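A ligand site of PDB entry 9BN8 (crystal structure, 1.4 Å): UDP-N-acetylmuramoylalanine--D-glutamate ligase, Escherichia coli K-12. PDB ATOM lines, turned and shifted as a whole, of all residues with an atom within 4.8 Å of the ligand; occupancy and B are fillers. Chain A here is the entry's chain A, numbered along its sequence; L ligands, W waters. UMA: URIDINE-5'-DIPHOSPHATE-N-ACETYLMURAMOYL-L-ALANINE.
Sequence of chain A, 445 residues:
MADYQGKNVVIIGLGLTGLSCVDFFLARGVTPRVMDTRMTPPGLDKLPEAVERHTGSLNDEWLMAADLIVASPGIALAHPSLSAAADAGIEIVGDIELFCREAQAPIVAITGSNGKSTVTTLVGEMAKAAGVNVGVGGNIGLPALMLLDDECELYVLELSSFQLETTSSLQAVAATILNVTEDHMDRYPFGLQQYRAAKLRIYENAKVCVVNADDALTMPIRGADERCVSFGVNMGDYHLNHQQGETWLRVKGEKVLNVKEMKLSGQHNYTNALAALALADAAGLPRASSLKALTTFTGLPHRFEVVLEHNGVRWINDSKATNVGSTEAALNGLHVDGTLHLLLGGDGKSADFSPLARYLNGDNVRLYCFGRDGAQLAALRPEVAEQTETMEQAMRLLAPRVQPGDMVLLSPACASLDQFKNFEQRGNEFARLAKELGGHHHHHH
N of Thr 37 is in hydrogen-bond range of O4 of the ligand (3.0 Å).
N3 of the ligand sits at hydrogen-bond distance from OG1 of Thr 37, 2.7 Å away.
The backbone NH (N) of Thr 17 lies within hydrogen-bond range of an oxygen (O2B) of the ligand, at 2.8 Å.
O2B of the ligand lies within hydrogen-bond range of OG1 of Thr 17, at 2.7 Å.
The backbone carbonyl oxygen of Asn 139 sits at hydrogen-bond distance from an oxygen (O4') of the ligand.
An oxygen (O3') of the ligand lies close to the side-chain amide oxygen (OD1) of Asn 139 (2.9 Å).
The backbone NH (N) of Gly 74 sits at hydrogen-bond distance from an oxygen (O2A) of the ligand.
O2' of the ligand is in hydrogen-bond range of O of Gly 74 (2.9 Å).
The guanidinium group of Arg 38 lies within salt-bridge range of an oxygen (O1A) of the ligand, at 3.5 Å.
NE2 of His 184 is in hydrogen-bond range of O19 of the ligand, 3.0 Å away.
The backbone NH (N) of Leu 16 lies within hydrogen-bond range of an oxygen (O1B) of the ligand (3.1 Å).
The side-chain amide nitrogen of Gln 163 is in hydrogen-bond range of an oxygen (O6') of the ligand, 3.1 Å away.
O6' of the ligand sits at hydrogen-bond distance from O of Gly 138 (3.1 Å).
N3 of the ligand lies close to OD1 of Asp 36, at 3.3 Å.
The guanidinium group of Arg 38 is in salt-bridge range of the side-chain carboxylate of Asp 36 (2.8 Å).
The side-chain carboxylate of Asp 183 sits at hydrogen-bond distance from a ring nitrogen (NE2) of His 184 (3.5 Å).
The side-chain amide oxygen (OE1) of Gln 163 is in hydrogen-bond range of the backbone NH (N) of Ser 160.
The side-chain hydroxyl of Ser 72 is in hydrogen-bond range of the backbone carbonyl oxygen of Ile 12 (2.7 Å).
The side-chain hydroxyl of Ser 160 lies close to the backbone NH of Phe 162, at 3.3 Å.
CG2 of Ile 12 touches O4 of the ligand, 3.8 Å away.
Gly 15 touches the ligand.
Ser 72 touches the ligand (CB to O2A, 3.2 Å).
Pro 73 touches the ligand (CG to O7', 3.4 Å).
Ile 75 touches the ligand (CD1 to O4, 3.9 Å).
Gly 141 touches the ligand (CA to O4', 3.4 Å).
CB of Ser 160 touches C23 of the ligand, at 3.6 Å.
Phe 162 touches the ligand.
Hydrophobic or aromatic side chains that line the ligand: Ile 12, Leu 16, Pro 73, Ile 75, Phe 162 and His 184.
Within 4 Å of the ligand: Ile 12, Gly 15, Leu 16, Thr 17, Asp 36, Thr 37, Arg 38, Ser 72, Pro 73, Gly 74, Ile 75, Gly 138, Asn 139, Gly 141, Ser 160, Phe 162, Gln 163 and His 184.
Water W4 lies within hydrogen-bond range of the side-chain hydroxyl of Thr 322 (2.6 Å), an oxygen (O19) of the ligand (2.7 Å) and the side-chain carboxylate of Asp 183 (2.7 Å).
Water W16 lies within hydrogen-bond range of the side-chain hydroxyl (OG) of Ser 160, the side-chain amide oxygen (OD1) of Asn 139 and an oxygen (O7') of the ligand.
Water W7 bridges an oxygen (O20) of the ligand (2.8 Å) and the side-chain amino group (NZ) of Lys 116 (3.2 Å).
Water W10 lies within hydrogen-bond range of the side-chain hydroxyl of Ser 72 (2.8 Å), an oxygen (O1A) of the ligand (2.8 Å), the backbone NH of Gly 15 (2.8 Å) and the backbone NH of Gly 18 (2.9 Å).
Water W11 bridges OD2 of Asp 95 (2.8 Å) and O6' of the ligand (2.8 Å).
Water W6 lies within hydrogen-bond range of O2' of the ligand (3.4 Å) and O of Gly 74 (3.5 Å).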
ATOM      1  N   ILE A  12      11.712 -14.730  16.263  1.00  0.00           N
ATOM      2  CA  ILE A  12      11.976 -16.146  16.546  1.00  0.00           C
ATOM      3  C   ILE A  12      10.985 -16.966  15.744  1.00  0.00           C
ATOM      4  O   ILE A  12       9.766 -16.836  15.923  1.00  0.00           O
ATOM      5  CB  ILE A  12      11.869 -16.498  18.032  1.00  0.00           C
ATOM      6  CG1 ILE A  12      12.793 -15.637  18.884  1.00  0.00           C
ATOM      7  CG2 ILE A  12      12.198 -17.997  18.204  1.00  0.00           C
ATOM      8  CD1 ILE A  12      12.554 -15.819  20.344  1.00  0.00           C
ATOM      9  N   GLY A  13      11.510 -17.811  14.879  1.00  0.00           N
ATOM     10  CA  GLY A  13      10.725 -18.721  14.076  1.00  0.00           C
ATOM     11  C   GLY A  13      10.870 -18.416  12.602  1.00  0.00           C
ATOM     12  O   GLY A  13      10.663 -17.286  12.144  1.00  0.00           O
ATOM     13  N   GLY A  15       9.092 -20.225  10.279  1.00  0.00           N
ATOM     14  CA  GLY A  15       7.935 -20.804   9.660  1.00  0.00           C
ATOM     15  C   GLY A  15       7.093 -19.735   8.979  1.00  0.00           C
ATOM     16  O   GLY A  15       7.567 -18.646   8.648  1.00  0.00           O
ATOM     17  N   LEU A  16       5.811 -20.041   8.811  1.00  0.00           N
ATOM     18  CA  LEU A  16       4.925 -19.124   8.121  1.00  0.00           C
ATOM     19  C   LEU A  16       4.837 -17.801   8.855  1.00  0.00           C
ATOM     20  O   LEU A  16       4.844 -16.724   8.235  1.00  0.00           O
ATOM     21  CB  LEU A  16       3.522 -19.725   8.033  1.00  0.00           C
ATOM     22  CG  LEU A  16       3.342 -21.022   7.255  1.00  0.00           C
ATOM     23  CD1 LEU A  16       1.891 -21.493   7.354  1.00  0.00           C
ATOM     24  CD2 LEU A  16       3.769 -20.823   5.802  1.00  0.00           C
ATOM     25  N   THR A  17       4.721 -17.857  10.173  1.00  0.00           N
ATOM     26  CA  THR A  17       4.579 -16.642  10.949  1.00  0.00           C
ATOM     27  C   THR A  17       5.826 -15.781  10.818  1.00  0.00           C
ATOM     28  O   THR A  17       5.749 -14.575  10.585  1.00  0.00           O
ATOM     29  CB  THR A  17       4.338 -16.966  12.413  1.00  0.00           C
ATOM     30  OG1 THR A  17       3.136 -17.718  12.543  1.00  0.00           O
ATOM     31  CG2 THR A  17       4.209 -15.704  13.218  1.00  0.00           C
ATOM     32  N   GLY A  18       7.000 -16.390  11.027  1.00  0.00           N
ATOM     33  CA  GLY A  18       8.219 -15.634  11.023  1.00  0.00           C
ATOM     34  C   GLY A  18       8.458 -14.950   9.696  1.00  0.00           C
ATOM     35  O   GLY A  18       8.891 -13.791   9.640  1.00  0.00           O
ATOM     36  N   MET A  35      15.865 -15.881  14.050  1.00  0.00           N
ATOM     37  CA  MET A  35      16.503 -17.097  14.547  1.00  0.00           C
ATOM     38  C   MET A  35      15.454 -18.205  14.689  1.00  0.00           C
ATOM     39  O   MET A  35      14.252 -17.948  14.779  1.00  0.00           O
ATOM     40  CB  MET A  35      17.176 -16.847  15.903  1.00  0.00           C
ATOM     41  CG  MET A  35      16.188 -16.530  17.003  1.00  0.00           C
ATOM     42  SD  MET A  35      16.956 -16.165  18.608  1.00  0.00           S
ATOM     43  CE  MET A  35      17.897 -14.729  18.180  1.00  0.00           C
ATOM     44  N   ASP A  36      15.929 -19.447  14.775  1.00  0.00           N
ATOM     45  CA  ASP A  36      15.055 -20.595  14.964  1.00  0.00           C
ATOM     46  C   ASP A  36      15.895 -21.698  15.599  1.00  0.00           C
ATOM     47  O   ASP A  36      17.065 -21.861  15.218  1.00  0.00           O
ATOM     48  CB  ASP A  36      14.518 -21.057  13.592  1.00  0.00           C
ATOM     49  CG  ASP A  36      13.339 -22.024  13.698  1.00  0.00           C
ATOM     50  OD1 ASP A  36      13.514 -23.159  14.196  1.00  0.00           O
ATOM     51  OD2 ASP A  36      12.219 -21.651  13.286  1.00  0.00           O
ATOM     52  N   THR A  37      15.316 -22.455  16.542  1.00  0.00           N
ATOM     53  CA  THR A  37      16.081 -23.508  17.201  1.00  0.00           C
ATOM     54  C   THR A  37      16.349 -24.689  16.277  1.00  0.00           C
ATOM     55  O   THR A  37      17.260 -25.479  16.546  1.00  0.00           O
ATOM     56  CB  THR A  37      15.402 -24.055  18.471  1.00  0.00           C
ATOM     57  OG1 THR A  37      14.155 -24.674  18.162  1.00  0.00           O
ATOM     58  CG2 THR A  37      15.186 -22.973  19.499  1.00  0.00           C
ATOM     59  N   ARG A  38      15.568 -24.856  15.214  1.00  0.00           N
ATOM     60  CA  ARG A  38      15.743 -25.986  14.315  1.00  0.00           C
ATOM     61  C   ARG A  38      16.965 -25.748  13.449  1.00  0.00           C
ATOM     62  O   ARG A  38      17.273 -24.606  13.087  1.00  0.00           O
ATOM     63  CB  ARG A  38      14.515 -26.163  13.430  1.00  0.00           C
ATOM     64  CG  ARG A  38      13.257 -26.566  14.188  1.00  0.00           C
ATOM     65  CD  ARG A  38      12.009 -26.421  13.325  1.00  0.00           C
ATOM     66  NE  ARG A  38      11.563 -25.032  13.203  1.00  0.00           N
ATOM     67  CZ  ARG A  38      10.458 -24.636  12.590  1.00  0.00           C
ATOM     68  NH1 ARG A  38       9.632 -25.504  12.028  1.00  0.00           N
ATOM     69  NH2 ARG A  38      10.160 -23.341  12.548  1.00  0.00           N
ATOM     70  N   LEU A  58      18.620 -20.765  19.928  1.00  0.00           N
ATOM     71  CA  LEU A  58      18.365 -19.344  20.128  1.00  0.00           C
ATOM     72  C   LEU A  58      19.685 -18.654  20.455  1.00  0.00           C
ATOM     73  O   LEU A  58      20.488 -19.166  21.219  1.00  0.00           O
ATOM     74  CB  LEU A  58      17.340 -19.116  21.233  1.00  0.00           C
ATOM     75  CG  LEU A  58      15.955 -19.693  20.968  1.00  0.00           C
ATOM     76  CD1 LEU A  58      14.973 -19.126  21.980  1.00  0.00           C
ATOM     77  CD2 LEU A  58      15.447 -19.405  19.573  1.00  0.00           C
ATOM     78  N   SER A  72       7.251 -16.326  17.330  1.00  0.00           N
ATOM     79  CA  SER A  72       6.264 -17.155  16.671  1.00  0.00           C
ATOM     80  C   SER A  72       5.572 -18.017  17.726  1.00  0.00           C
ATOM     81  O   SER A  72       6.140 -18.313  18.784  1.00  0.00           O
ATOM     82  CB  SER A  72       6.952 -18.049  15.649  1.00  0.00           C
ATOM     83  OG  SER A  72       7.482 -17.327  14.562  1.00  0.00           O
ATOM     84  N   PRO A  73       4.353 -18.476  17.439  1.00  0.00           N
ATOM     85  CA  PRO A  73       3.629 -19.270  18.436  1.00  0.00           C
ATOM     86  C   PRO A  73       4.297 -20.591  18.768  1.00  0.00           C
ATOM     87  O   PRO A  73       4.083 -21.117  19.860  1.00  0.00           O
ATOM     88  CB  PRO A  73       2.235 -19.456  17.813  1.00  0.00           C
ATOM     89  CG  PRO A  73       2.450 -19.264  16.327  1.00  0.00           C
ATOM     90  CD  PRO A  73       3.524 -18.188  16.249  1.00  0.00           C
ATOM     91  N   GLY A  74       5.142 -21.119  17.882  1.00  0.00           N
ATOM     92  CA  GLY A  74       5.811 -22.389  18.097  1.00  0.00           C
ATOM     93  C   GLY A  74       6.986 -22.379  19.039  1.00  0.00           C
ATOM     94  O   GLY A  74       7.532 -23.453  19.301  1.00  0.00           O
ATOM     95  N   ILE A  75       7.417 -21.230  19.564  1.00  0.00           N
ATOM     96  CA  ILE A  75       8.475 -21.167  20.574  1.00  0.00           C
ATOM     97  C   ILE A  75       7.818 -20.873  21.918  1.00  0.00           C
ATOM     98  O   ILE A  75       6.996 -19.963  22.034  1.00  0.00           O
ATOM     99  CB  ILE A  75       9.578 -20.152  20.201  1.00  0.00           C
ATOM    100  CG1 ILE A  75      10.796 -20.281  21.115  1.00  0.00           C
ATOM    101  CG2 ILE A  75       9.082 -18.727  20.292  1.00  0.00           C
ATOM    102  CD1 ILE A  75      11.676 -21.469  20.812  1.00  0.00           C
ATOM    103  N   ASP A  95       2.915 -12.168  16.326  1.00  0.00           N
ATOM    104  CA  ASP A  95       2.372 -11.560  15.118  1.00  0.00           C
ATOM    105  C   ASP A  95       0.965 -11.036  15.310  1.00  0.00           C
ATOM    106  O   ASP A  95       0.595 -10.022  14.701  1.00  0.00           O
ATOM    107  CB  ASP A  95       2.429 -12.509  13.909  1.00  0.00           C
ATOM    108  CG  ASP A  95       1.486 -13.699  14.024  1.00  0.00           C
ATOM    109  OD1 ASP A  95       1.437 -14.360  15.080  1.00  0.00           O
ATOM    110  OD2 ASP A  95       0.814 -13.998  13.020  1.00  0.00           O
ATOM    111  N   LYS A 116     -12.755 -24.265  16.033  1.00  0.00           N
ATOM    112  CA  LYS A 116     -12.402 -22.867  15.793  1.00  0.00           C
ATOM    113  C   LYS A 116     -12.257 -22.555  14.307  1.00  0.00           C
ATOM    114  O   LYS A 116     -12.665 -21.476  13.871  1.00  0.00           O
ATOM    115  CB  LYS A 116     -11.214 -22.394  16.619  1.00  0.00           C
ATOM    116  CG  LYS A 116      -9.965 -23.160  16.507  1.00  0.00           C
ATOM    117  CD  LYS A 116      -8.912 -22.592  17.494  1.00  0.00           C
ATOM    118  CE  LYS A 116      -7.695 -23.384  17.376  1.00  0.00           C
ATOM    119  NZ  LYS A 116      -7.934 -24.708  18.006  1.00  0.00           N
ATOM    120  N   GLY A 138      -5.174 -15.963  10.622  1.00  0.00           N
ATOM    121  CA  GLY A 138      -4.676 -16.377  11.900  1.00  0.00           C
ATOM    122  C   GLY A 138      -4.264 -17.831  11.876  1.00  0.00           C
ATOM    123  O   GLY A 138      -3.672 -18.311  10.908  1.00  0.00           O
ATOM    124  N   ASN A 139      -4.582 -18.531  12.971  1.00  0.00           N
ATOM    125  CA  ASN A 139      -4.154 -19.911  13.140  1.00  0.00           C
ATOM    126  C   ASN A 139      -4.722 -20.817  12.070  1.00  0.00           C
ATOM    127  O   ASN A 139      -4.193 -21.930  11.869  1.00  0.00           O
ATOM    128  CB  ASN A 139      -4.564 -20.367  14.544  1.00  0.00           C
ATOM    129  CG  ASN A 139      -3.947 -21.713  14.928  1.00  0.00           C
ATOM    130  OD1 ASN A 139      -2.741 -21.799  15.124  1.00  0.00           O
ATOM    131  ND2 ASN A 139      -4.765 -22.731  15.087  1.00  0.00           N
ATOM    132  N   ILE A 140      -5.799 -20.401  11.402  1.00  0.00           N
ATOM    133  CA  ILE A 140      -6.408 -21.181  10.326  1.00  0.00           C
ATOM    134  C   ILE A 140      -5.448 -21.395   9.182  1.00  0.00           C
ATOM    135  O   ILE A 140      -5.635 -22.314   8.386  1.00  0.00           O
ATOM    136  CB  ILE A 140      -7.731 -20.490   9.897  1.00  0.00           C
ATOM    137  CG1 ILE A 140      -8.571 -21.437   9.040  1.00  0.00           C
ATOM    138  CG2 ILE A 140      -7.431 -19.184   9.163  1.00  0.00           C
ATOM    139  CD1 ILE A 140      -9.981 -20.977   8.894  1.00  0.00           C
ATOM    140  N   GLY A 141      -4.408 -20.563   9.046  1.00  0.00           N
ATOM    141  CA  GLY A 141      -3.353 -20.854   8.101  1.00  0.00           C
ATOM    142  C   GLY A 141      -2.858 -19.714   7.245  1.00  0.00           C
ATOM    143  O   GLY A 141      -1.829 -19.845   6.581  1.00  0.00           O
ATOM    144  N   PRO A 143      -1.343 -16.175   7.681  1.00  0.00           N
ATOM    145  CA  PRO A 143      -0.838 -15.313   8.750  1.00  0.00           C
ATOM    146  C   PRO A 143      -1.539 -13.967   8.782  1.00  0.00           C
ATOM    147  O   PRO A 143      -1.696 -13.307   7.754  1.00  0.00           O
ATOM    148  CB  PRO A 143       0.649 -15.182   8.418  1.00  0.00           C
ATOM    149  CG  PRO A 143       0.973 -16.444   7.717  1.00  0.00           C
ATOM    150  CD  PRO A 143      -0.239 -16.751   6.893  1.00  0.00           C
ATOM    151  N   SER A 160      -4.888 -19.365  18.490  1.00  0.00           N
ATOM    152  CA  SER A 160      -4.490 -20.443  19.373  1.00  0.00           C
ATOM    153  C   SER A 160      -4.115 -19.901  20.739  1.00  0.00           C
ATOM    154  O   SER A 160      -3.869 -18.707  20.932  1.00  0.00           O
ATOM    155  CB  SER A 160      -3.264 -21.135  18.802  1.00  0.00           C
ATOM    156  OG  SER A 160      -2.146 -20.249  18.838  1.00  0.00           O
ATOM    157  N   PHE A 162      -1.271 -20.402  22.064  1.00  0.00           N
ATOM    158  CA  PHE A 162       0.091 -19.892  21.899  1.00  0.00           C
ATOM    159  C   PHE A 162       0.077 -18.447  21.438  1.00  0.00           C
ATOM    160  O   PHE A 162       0.821 -17.605  21.952  1.00  0.00           O
ATOM    161  CB  PHE A 162       0.854 -20.729  20.860  1.00  0.00           C
ATOM    162  CG  PHE A 162       0.981 -22.203  21.168  1.00  0.00           C
ATOM    163  CD1 PHE A 162       0.948 -22.708  22.460  1.00  0.00           C
ATOM    164  CD2 PHE A 162       1.180 -23.084  20.122  1.00  0.00           C
ATOM    165  CE1 PHE A 162       1.096 -24.076  22.683  1.00  0.00           C
ATOM    166  CE2 PHE A 162       1.330 -24.439  20.345  1.00  0.00           C
ATOM    167  CZ  PHE A 162       1.286 -24.928  21.630  1.00  0.00           C
ATOM    168  N   GLN A 163      -0.753 -18.141  20.433  1.00  0.00           N
ATOM    169  CA  GLN A 163      -0.829 -16.767  19.938  1.00  0.00           C
ATOM    170  C   GLN A 163      -1.352 -15.827  21.010  1.00  0.00           C
ATOM    171  O   GLN A 163      -0.871 -14.697  21.159  1.00  0.00           O
ATOM    172  CB  GLN A 163      -1.745 -16.698  18.716  1.00  0.00           C
ATOM    173  CG  GLN A 163      -1.134 -17.310  17.485  1.00  0.00           C
ATOM    174  CD  GLN A 163      -2.131 -17.569  16.380  1.00  0.00           C
ATOM    175  OE1 GLN A 163      -3.283 -17.894  16.628  1.00  0.00           O
ATOM    176  NE2 GLN A 163      -1.685 -17.425  15.149  1.00  0.00           N
ATOM    177  N   ASP A 183      -5.196 -30.102  25.453  1.00  0.00           N
ATOM    178  CA  ASP A 183      -4.362 -30.062  24.260  1.00  0.00           C
ATOM    179  C   ASP A 183      -3.077 -29.348  24.635  1.00  0.00           C
ATOM    180  O   ASP A 183      -3.038 -28.603  25.618  1.00  0.00           O
ATOM    181  CB  ASP A 183      -5.085 -29.359  23.105  1.00  0.00           C
ATOM    182  CG  ASP A 183      -4.474 -29.676  21.723  1.00  0.00           C
ATOM    183  OD1 ASP A 183      -3.479 -30.425  21.610  1.00  0.00           O
ATOM    184  OD2 ASP A 183      -5.052 -29.175  20.732  1.00  0.00           O
ATOM    185  N   HIS A 184      -2.021 -29.579  23.851  1.00  0.00           N
ATOM    186  CA  HIS A 184      -0.758 -28.852  24.002  1.00  0.00           C
ATOM    187  C   HIS A 184      -0.165 -28.978  25.395  1.00  0.00           C
ATOM    188  O   HIS A 184       0.529 -28.074  25.865  1.00  0.00           O
ATOM    189  CB  HIS A 184      -0.937 -27.378  23.629  1.00  0.00           C
ATOM    190  CG  HIS A 184      -1.427 -27.205  22.237  1.00  0.00           C
ATOM    191  ND1 HIS A 184      -0.746 -27.713  21.160  1.00  0.00           N
ATOM    192  CD2 HIS A 184      -2.565 -26.658  21.749  1.00  0.00           C
ATOM    193  CE1 HIS A 184      -1.420 -27.449  20.051  1.00  0.00           C
ATOM    194  NE2 HIS A 184      -2.525 -26.807  20.383  1.00  0.00           N
ATOM    195  N   THR A 322      -6.518 -33.277  15.936  1.00  0.00           N
ATOM    196  CA  THR A 322      -5.188 -33.304  16.530  1.00  0.00           C
ATOM    197  C   THR A 322      -5.229 -33.357  18.055  1.00  0.00           C
ATOM    198  O   THR A 322      -4.189 -33.229  18.691  1.00  0.00           O
ATOM    199  CB  THR A 322      -4.402 -32.079  16.076  1.00  0.00           C
ATOM    200  OG1 THR A 322      -5.201 -30.911  16.323  1.00  0.00           O
ATOM    201  CG2 THR A 322      -4.059 -32.177  14.584  1.00  0.00           C
ATOM    202  N   LEU A 417       3.339 -33.935  13.450  1.00  0.00           N
ATOM    203  CA  LEU A 417       4.669 -33.392  13.206  1.00  0.00           C
ATOM    204  C   LEU A 417       5.799 -34.401  13.404  1.00  0.00           C
ATOM    205  O   LEU A 417       6.913 -34.125  12.961  1.00  0.00           O
ATOM    206  CB  LEU A 417       4.886 -32.150  14.066  1.00  0.00           C
ATOM    207  CG  LEU A 417       4.703 -32.381  15.561  1.00  0.00           C
ATOM    208  CD1 LEU A 417       6.020 -32.699  16.193  1.00  0.00           C
ATOM    209  CD2 LEU A 417       4.039 -31.163  16.201  1.00  0.00           C
ATOM    210  N   PHE A 423      -0.820 -31.471   9.382  1.00  0.00           N
ATOM    211  CA  PHE A 423      -1.992 -32.321   9.277  1.00  0.00           C
ATOM    212  C   PHE A 423      -2.543 -32.355   7.869  1.00  0.00           C
ATOM    213  O   PHE A 423      -3.225 -33.326   7.490  1.00  0.00           O
ATOM    214  CB  PHE A 423      -3.068 -31.895  10.297  1.00  0.00           C
ATOM    215  CG  PHE A 423      -3.775 -30.604   9.955  1.00  0.00           C
ATOM    216  CD1 PHE A 423      -4.840 -30.597   9.054  1.00  0.00           C
ATOM    217  CD2 PHE A 423      -3.399 -29.415  10.539  1.00  0.00           C
ATOM    218  CE1 PHE A 423      -5.486 -29.413   8.729  1.00  0.00           C
ATOM    219  CE2 PHE A 423      -4.061 -28.229  10.215  1.00  0.00           C
ATOM    220  CZ  PHE A 423      -5.089 -28.240   9.303  1.00  0.00           C
HETATM  221  N1  UMA L   1       9.789 -24.504  16.237  1.00  0.00           N
HETATM  222  C2  UMA L   1      11.010 -24.847  16.789  1.00  0.00           C
HETATM  223  N3  UMA L   1      11.862 -23.804  17.034  1.00  0.00           N
HETATM  224  C4  UMA L   1      11.639 -22.471  16.791  1.00  0.00           C
HETATM  225  C5  UMA L   1      10.354 -22.178  16.225  1.00  0.00           C
HETATM  226  C6  UMA L   1       9.494 -23.177  15.975  1.00  0.00           C
HETATM  227  O2  UMA L   1      11.290 -26.008  17.036  1.00  0.00           O
HETATM  228  O4  UMA L   1      12.511 -21.643  17.020  1.00  0.00           O
HETATM  229  C1B UMA L   1       8.789 -25.517  15.939  1.00  0.00           C
HETATM  230  C2B UMA L   1       7.560 -25.457  16.870  1.00  0.00           C
HETATM  231  O2' UMA L   1       7.767 -26.118  18.078  1.00  0.00           O
HETATM  232  C3B UMA L   1       6.427 -25.998  16.009  1.00  0.00           C
HETATM  233  C4B UMA L   1       6.903 -25.642  14.602  1.00  0.00           C
HETATM  234  O4B UMA L   1       8.287 -25.273  14.665  1.00  0.00           O
HETATM  235  O3B UMA L   1       6.308 -27.403  16.133  1.00  0.00           O
HETATM  236  C5B UMA L   1       6.099 -24.514  13.964  1.00  0.00           C
HETATM  237  O5B UMA L   1       6.175 -23.350  14.755  1.00  0.00           O
HETATM  238  PA  UMA L   1       5.977 -21.896  14.021  1.00  0.00           P
HETATM  239  O1A UMA L   1       7.116 -21.634  13.105  1.00  0.00           O
HETATM  240  O2A UMA L   1       5.620 -20.936  15.110  1.00  0.00           O
HETATM  241  O3A UMA L   1       4.668 -22.256  13.142  1.00  0.00           O
HETATM  242  PB  UMA L   1       4.164 -21.485  11.800  1.00  0.00           P
HETATM  243  O1B UMA L   1       4.591 -22.237  10.605  1.00  0.00           O
HETATM  244  O2B UMA L   1       4.450 -20.037  11.890  1.00  0.00           O
HETATM  245  O1' UMA L   1       2.582 -21.769  12.000  1.00  0.00           O
HETATM  246  C1' UMA L   1       1.895 -21.088  13.009  1.00  0.00           C
HETATM  247  C2' UMA L   1       0.887 -22.061  13.646  1.00  0.00           C
HETATM  248  N2' UMA L   1       1.593 -23.170  14.214  1.00  0.00           N
HETATM  249  C7' UMA L   1       1.779 -23.299  15.540  1.00  0.00           C
HETATM  250  O7' UMA L   1       1.320 -22.509  16.354  1.00  0.00           O
HETATM  251  C8' UMA L   1       2.570 -24.499  15.952  1.00  0.00           C
HETATM  252  C3' UMA L   1      -0.108 -22.448  12.570  1.00  0.00           C
HETATM  253  O3' UMA L   1      -1.174 -23.200  13.095  1.00  0.00           O
HETATM  254  C4' UMA L   1      -0.747 -21.182  12.013  1.00  0.00           C
HETATM  255  O4' UMA L   1      -1.613 -21.503  10.941  1.00  0.00           O
HETATM  256  C5' UMA L   1       0.272 -20.191  11.486  1.00  0.00           C
HETATM  257  O5' UMA L   1       1.262 -19.965  12.472  1.00  0.00           O
HETATM  258  C6' UMA L   1      -0.319 -18.840  11.128  1.00  0.00           C
HETATM  259  O6' UMA L   1      -0.845 -18.164  12.255  1.00  0.00           O
HETATM  260  C18 UMA L   1      -1.071 -24.592  12.932  1.00  0.00           C
HETATM  261  C19 UMA L   1      -1.100 -25.332  14.270  1.00  0.00           C
HETATM  262  O18 UMA L   1      -0.757 -26.490  14.345  1.00  0.00           O
HETATM  263  C20 UMA L   1      -2.259 -25.079  12.105  1.00  0.00           C
HETATM  264  N4  UMA L   1      -1.501 -24.609  15.307  1.00  0.00           N
HETATM  265  C21 UMA L   1      -1.645 -25.195  16.618  1.00  0.00           C
HETATM  266  C22 UMA L   1      -3.002 -25.959  16.645  1.00  0.00           C
HETATM  267  O19 UMA L   1      -3.134 -26.899  17.441  1.00  0.00           O
HETATM  268  O20 UMA L   1      -3.922 -25.570  15.873  1.00  0.00           O
HETATM  269  C23 UMA L   1      -1.588 -24.191  17.741  1.00  0.00           C
HETATM  270  O   HOH W   1      -2.480 -28.727  14.549  1.00  0.00           O
HETATM  271  O   HOH W   2       4.057 -27.663  14.399  1.00  0.00           O
HETATM  272  O   HOH W   3       2.445 -23.892   9.616  1.00  0.00           O
HETATM  273  O   HOH W   4      -4.217 -29.293  18.125  1.00  0.00           O
HETATM  274  O   HOH W   5       8.078 -29.250  14.499  1.00  0.00           O
HETATM  275  O   HOH W   6       5.450 -25.924  20.547  1.00  0.00           O
HETATM  276  O   HOH W   7      -6.040 -27.089  16.897  1.00  0.00           O
HETATM  277  O   HOH W   8       2.537 -25.258  12.285  1.00  0.00           O
HETATM  278  O   HOH W   9       6.585 -24.164  10.200  1.00  0.00           O
HETATM  279  O   HOH W  10       7.589 -18.958  12.316  1.00  0.00           O
HETATM  280  O   HOH W  11      -1.430 -15.377  12.218  1.00  0.00           O
HETATM  281  O   HOH W  12       1.382 -28.073  14.909  1.00  0.00           O
HETATM  282  O   HOH W  13       1.002 -17.001  14.192  1.00  0.00           O
HETATM  283  O   HOH W  14      -0.446 -23.309   9.063  1.00  0.00           O
HETATM  284  O   HOH W  15       0.024 -27.399  11.795  1.00  0.00           O
HETATM  285  O   HOH W  16      -0.750 -20.657  16.623  1.00  0.00           O
